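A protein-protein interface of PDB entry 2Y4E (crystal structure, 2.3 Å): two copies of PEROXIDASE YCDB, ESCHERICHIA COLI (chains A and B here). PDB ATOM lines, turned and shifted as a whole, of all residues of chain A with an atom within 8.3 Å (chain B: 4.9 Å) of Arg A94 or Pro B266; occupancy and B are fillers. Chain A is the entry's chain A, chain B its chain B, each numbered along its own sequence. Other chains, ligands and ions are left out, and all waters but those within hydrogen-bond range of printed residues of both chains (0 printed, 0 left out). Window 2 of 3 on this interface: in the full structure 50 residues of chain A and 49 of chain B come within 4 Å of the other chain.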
ATOM      1  N   THR A  90      27.835  19.643   0.447  1.00  0.00           N
ATOM      2  CA  THR A  90      26.704  18.748   0.635  1.00  0.00           C
ATOM      3  C   THR A  90      26.462  17.965  -0.657  1.00  0.00           C
ATOM      4  O   THR A  90      25.765  18.452  -1.555  1.00  0.00           O
ATOM      5  CB  THR A  90      25.420  19.519   1.042  1.00  0.00           C
ATOM      6  OG1 THR A  90      25.144  20.533   0.075  1.00  0.00           O
ATOM      7  CG2 THR A  90      25.613  20.186   2.362  1.00  0.00           C
ATOM      8  N   PRO A  91      27.032  16.749  -0.748  1.00  0.00           N
ATOM      9  CA  PRO A  91      26.969  15.986  -2.008  1.00  0.00           C
ATOM     10  C   PRO A  91      25.548  15.463  -2.323  1.00  0.00           C
ATOM     11  O   PRO A  91      25.157  15.399  -3.497  1.00  0.00           O
ATOM     12  CB  PRO A  91      27.950  14.838  -1.767  1.00  0.00           C
ATOM     13  CG  PRO A  91      27.870  14.593  -0.262  1.00  0.00           C
ATOM     14  CD  PRO A  91      27.560  15.942   0.374  1.00  0.00           C
ATOM     15  N   ASN A  92      24.785  15.125  -1.279  1.00  0.00           N
ATOM     16  CA  ASN A  92      23.392  14.678  -1.425  1.00  0.00           C
ATOM     17  C   ASN A  92      22.394  15.766  -1.006  1.00  0.00           C
ATOM     18  O   ASN A  92      22.063  15.896   0.178  1.00  0.00           O
ATOM     19  CB  ASN A  92      23.154  13.377  -0.647  1.00  0.00           C
ATOM     20  CG  ASN A  92      21.700  12.929  -0.681  1.00  0.00           C
ATOM     21  OD1 ASN A  92      20.898  13.409  -1.490  1.00  0.00           O
ATOM     22  ND2 ASN A  92      21.356  11.994   0.197  1.00  0.00           N
ATOM     23  N   PRO A  93      21.882  16.535  -1.983  1.00  0.00           N
ATOM     24  CA  PRO A  93      21.063  17.707  -1.678  1.00  0.00           C
ATOM     25  C   PRO A  93      19.636  17.396  -1.195  1.00  0.00           C
ATOM     26  O   PRO A  93      18.829  18.321  -1.015  1.00  0.00           O
ATOM     27  CB  PRO A  93      21.037  18.472  -3.001  1.00  0.00           C
ATOM     28  CG  PRO A  93      21.235  17.419  -4.055  1.00  0.00           C
ATOM     29  CD  PRO A  93      21.990  16.284  -3.433  1.00  0.00           C
ATOM     30  N   ARG A  94      19.326  16.120  -0.993  1.00  0.00           N
ATOM     31  CA  ARG A  94      18.061  15.736  -0.384  1.00  0.00           C
ATOM     32  C   ARG A  94      18.225  15.750   1.124  1.00  0.00           C
ATOM     33  O   ARG A  94      17.263  15.584   1.866  1.00  0.00           O
ATOM     34  CB  ARG A  94      17.597  14.357  -0.864  1.00  0.00           C
ATOM     35  CG  ARG A  94      17.129  14.301  -2.322  1.00  0.00           C
ATOM     36  CD  ARG A  94      16.475  12.946  -2.641  1.00  0.00           C
ATOM     37  NE  ARG A  94      17.346  11.811  -2.329  1.00  0.00           N
ATOM     38  CZ  ARG A  94      18.342  11.388  -3.110  1.00  0.00           C
ATOM     39  NH1 ARG A  94      18.596  11.977  -4.281  1.00  0.00           N
ATOM     40  NH2 ARG A  94      19.085  10.356  -2.727  1.00  0.00           N
ATOM     41  N   LEU A  95      19.460  15.948   1.564  1.00  0.00           N
ATOM     42  CA  LEU A  95      19.774  16.227   2.966  1.00  0.00           C
ATOM     43  C   LEU A  95      19.848  17.752   3.186  1.00  0.00           C
ATOM     44  O   LEU A  95      20.039  18.512   2.219  1.00  0.00           O
ATOM     45  CB  LEU A  95      21.120  15.592   3.333  1.00  0.00           C
ATOM     46  CG  LEU A  95      21.287  14.072   3.303  1.00  0.00           C
ATOM     47  CD1 LEU A  95      22.725  13.741   3.628  1.00  0.00           C
ATOM     48  CD2 LEU A  95      20.317  13.379   4.300  1.00  0.00           C
ATOM     49  N   PRO A  96      19.691  18.214   4.456  1.00  0.00           N
ATOM     50  CA  PRO A  96      19.924  19.643   4.720  1.00  0.00           C
ATOM     51  C   PRO A  96      21.363  20.002   4.373  1.00  0.00           C
ATOM     52  O   PRO A  96      22.234  19.141   4.447  1.00  0.00           O
ATOM     53  CB  PRO A  96      19.718  19.765   6.229  1.00  0.00           C
ATOM     54  CG  PRO A  96      18.854  18.609   6.604  1.00  0.00           C
ATOM     55  CD  PRO A  96      19.266  17.494   5.677  1.00  0.00           C
ATOM     56  N   PRO A  97      21.612  21.259   3.990  1.00  0.00           N
ATOM     57  CA  PRO A  97      22.996  21.645   3.766  1.00  0.00           C
ATOM     58  C   PRO A  97      23.829  21.417   5.029  1.00  0.00           C
ATOM     59  O   PRO A  97      23.349  21.635   6.132  1.00  0.00           O
ATOM     60  CB  PRO A  97      22.906  23.141   3.448  1.00  0.00           C
ATOM     61  CG  PRO A  97      21.458  23.441   3.223  1.00  0.00           C
ATOM     62  CD  PRO A  97      20.682  22.404   3.933  1.00  0.00           C
ATOM     63  N   LYS A 178      22.806  23.580  14.502  1.00  0.00           N
ATOM     64  CA  LYS A 178      22.491  22.530  13.538  1.00  0.00           C
ATOM     65  C   LYS A 178      22.949  21.172  14.071  1.00  0.00           C
ATOM     66  O   LYS A 178      22.303  20.144  13.846  1.00  0.00           O
ATOM     67  CB  LYS A 178      23.196  22.793  12.202  1.00  0.00           C
ATOM     68  CG  LYS A 178      22.736  21.853  11.102  1.00  0.00           C
ATOM     69  CD  LYS A 178      23.829  21.544  10.113  1.00  0.00           C
ATOM     70  CE  LYS A 178      23.644  20.123   9.518  1.00  0.00           C
ATOM     71  NZ  LYS A 178      22.550  20.008   8.526  1.00  0.00           N
ATOM     72  N   ARG B 264      17.473  22.916   8.758  1.00  0.00           N
ATOM     73  CA  ARG B 264      17.077  21.523   8.763  1.00  0.00           C
ATOM     74  C   ARG B 264      16.374  21.126   7.475  1.00  0.00           C
ATOM     75  O   ARG B 264      15.884  19.996   7.347  1.00  0.00           O
ATOM     76  CB  ARG B 264      16.163  21.238   9.940  1.00  0.00           C
ATOM     77  CG  ARG B 264      16.869  21.167  11.265  1.00  0.00           C
ATOM     78  CD  ARG B 264      15.908  20.701  12.302  1.00  0.00           C
ATOM     79  NE  ARG B 264      15.971  21.577  13.463  1.00  0.00           N
ATOM     80  CZ  ARG B 264      14.955  22.312  13.918  1.00  0.00           C
ATOM     81  NH1 ARG B 264      13.746  22.280  13.346  1.00  0.00           N
ATOM     82  NH2 ARG B 264      15.160  23.075  14.975  1.00  0.00           N
ATOM     83  N   THR B 265      16.330  22.035   6.514  1.00  0.00           N
ATOM     84  CA  THR B 265      15.547  21.806   5.314  1.00  0.00           C
ATOM     85  C   THR B 265      16.458  21.433   4.133  1.00  0.00           C
ATOM     86  O   THR B 265      17.424  22.128   3.882  1.00  0.00           O
ATOM     87  CB  THR B 265      14.699  23.034   5.008  1.00  0.00           C
ATOM     88  OG1 THR B 265      13.830  23.286   6.123  1.00  0.00           O
ATOM     89  CG2 THR B 265      13.872  22.843   3.738  1.00  0.00           C
ATOM     90  N   PRO B 266      16.150  20.317   3.421  1.00  0.00           N
ATOM     91  CA  PRO B 266      16.981  19.864   2.292  1.00  0.00           C
ATOM     92  C   PRO B 266      17.424  20.990   1.361  1.00  0.00           C
ATOM     93  O   PRO B 266      16.668  21.931   1.092  1.00  0.00           O
ATOM     94  CB  PRO B 266      16.085  18.862   1.562  1.00  0.00           C
ATOM     95  CG  PRO B 266      15.200  18.283   2.687  1.00  0.00           C
ATOM     96  CD  PRO B 266      15.115  19.323   3.789  1.00  0.00           C
ATOM     97  N   LEU B 267      18.668  20.890   0.893  1.00  0.00           N
ATOM     98  CA  LEU B 267      19.241  21.905   0.021  1.00  0.00           C
ATOM     99  C   LEU B 267      18.392  22.020  -1.240  1.00  0.00           C
ATOM    100  O   LEU B 267      18.067  23.122  -1.694  1.00  0.00           O
ATOM    101  CB  LEU B 267      20.703  21.579  -0.297  1.00  0.00           C
ATOM    102  CG  LEU B 267      21.374  22.472  -1.356  1.00  0.00           C
ATOM    103  CD1 LEU B 267      21.347  23.942  -0.980  1.00  0.00           C
ATOM    104  CD2 LEU B 267      22.823  22.020  -1.621  1.00  0.00           C
ATOM    105  N   LYS B 268      18.012  20.864  -1.772  1.00  0.00           N
ATOM    106  CA  LYS B 268      17.121  20.777  -2.924  1.00  0.00           C
ATOM    107  C   LYS B 268      15.860  21.577  -2.667  1.00  0.00           C
ATOM    108  O   LYS B 268      15.442  22.368  -3.534  1.00  0.00           O
ATOM    109  CB  LYS B 268      16.766  19.321  -3.203  1.00  0.00           C
ATOM    110  CG  LYS B 268      16.516  19.037  -4.666  1.00  0.00           C
ATOM    111  CD  LYS B 268      16.501  17.532  -4.921  1.00  0.00           C
ATOM    112  CE  LYS B 268      15.138  16.949  -4.616  1.00  0.00           C
ATOM    113  NZ  LYS B 268      14.181  17.400  -5.648  1.00  0.00           N
ATOM    114  N   GLU B 269      15.277  21.396  -1.476  1.00  0.00           N
ATOM    115  CA  GLU B 269      14.071  22.130  -1.119  1.00  0.00           C
ATOM    116  C   GLU B 269      14.361  23.613  -1.001  1.00  0.00           C
ATOM    117  O   GLU B 269      13.604  24.447  -1.528  1.00  0.00           O
ATOM    118  CB  GLU B 269      13.422  21.621   0.163  1.00  0.00           C
ATOM    119  CG  GLU B 269      12.005  22.179   0.347  1.00  0.00           C
ATOM    120  CD  GLU B 269      11.324  21.730   1.639  1.00  0.00           C
ATOM    121  OE1 GLU B 269      11.794  20.753   2.291  1.00  0.00           O
ATOM    122  OE2 GLU B 269      10.295  22.350   2.000  1.00  0.00           O
ATOM    123  N   GLN B 270      15.459  23.943  -0.322  1.00  0.00           N
ATOM    124  CA  GLN B 270      15.893  25.340  -0.236  1.00  0.00           C
ATOM    125  C   GLN B 270      15.991  25.969  -1.619  1.00  0.00           C
ATOM    126  O   GLN B 270      15.502  27.082  -1.839  1.00  0.00           O
ATOM    127  CB  GLN B 270      17.224  25.453   0.493  1.00  0.00           C
ATOM    128  CG  GLN B 270      17.161  25.210   2.015  1.00  0.00           C
ATOM    129  CD  GLN B 270      18.461  25.622   2.685  1.00  0.00           C
ATOM    130  OE1 GLN B 270      19.323  26.242   2.054  1.00  0.00           O
ATOM    131  NE2 GLN B 270      18.613  25.279   3.962  1.00  0.00           N
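O of Leu A95 lies within hydrogen-bond range of N of Leu B267 (3.0 Å). The backbone carbonyl oxygen (O) of Pro A93 sits at hydrogen-bond distance from the backbone NH (N) of Lys B268 (2.8 Å). The backbone carbonyl oxygen of Pro A93 lies within hydrogen-bond range of the backbone NH of Leu B267, at 3.2 Å.
The side-chain amide nitrogen (NE2) of Gln B270 sits at hydrogen-bond distance from the backbone carbonyl oxygen (O) of Thr B265 (3.4 Å). The side-chain amide oxygen of Asn A92 lies close to the backbone NH of Arg A94. The backbone carbonyl oxygen (O) of Pro A97 lies within hydrogen-bond range of the side-chain amino group (NZ) of Lys A178, 3.0 Å away.
CD2 of Leu B267 touches OG1 of Thr A90, at 3.2 Å. O of Pro A93 touches CB of Pro B266, at 3.8 Å. O of Arg A94 touches CG of Pro B266, 3.5 Å away. CA of Pro B266 touches O of Leu A95 (3.3 Å). O of Arg B264 touches CG of Pro A96, at 3.4 Å. O of Thr B265 touches CA of Pro A96, at 3.6 Å. Pro B266 touches Pro A96. Pro A97 touches Thr B265. Leu B267 touches Pro A97. CG of Pro A97 touches NE2 of Gln B270 (3.5 Å).
Printed residues of chain B within 4 Å of Thr A90: Leu B267. Asn A92 touches none of the printed residues of chain B. Of chain B, only Pro B266 comes within 4 Å of Arg A94. Of the printed residues of chain B, Pro A97 touches Thr B265 (3.3 Å), Leu B267 (3.9 Å) and Gln B270 (3.5 Å). Lys A178 touches none of the printed residues of chain B. Of the printed residues of chain A, Thr B265 touches Pro A96 (3.6 Å) and Pro A97 (3.3 Å). Pro B266 touches just these residues of chain A: Pro A93 (3.8 Å), Arg A94 (3.5 Å), Leu A95 (3.3 Å) and Pro A96 (3.8 Å). Printed residues of chain A within 4 Å of Gln B270: Pro A97 (3.5 Å). The nearest printed residue of chain A that does not touch Leu B267 is Pro A96 (4.2 Å).
Hydrophobic or aromatic side chains of chain B within 4 Å of the printed part of chain A: Pro B266 and Leu B267. Among the printed residues, 13 pairs touch across the chains. Among the printed residues, no Asp or Glu carboxylate lies within 4 Å of a Lys or Arg side-chain nitrogen of the other chain.
No position is printed for both chains. Of the 13 pairs that touch across the chains among the printed residues, none has its exchanged pair printed and touching as well.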
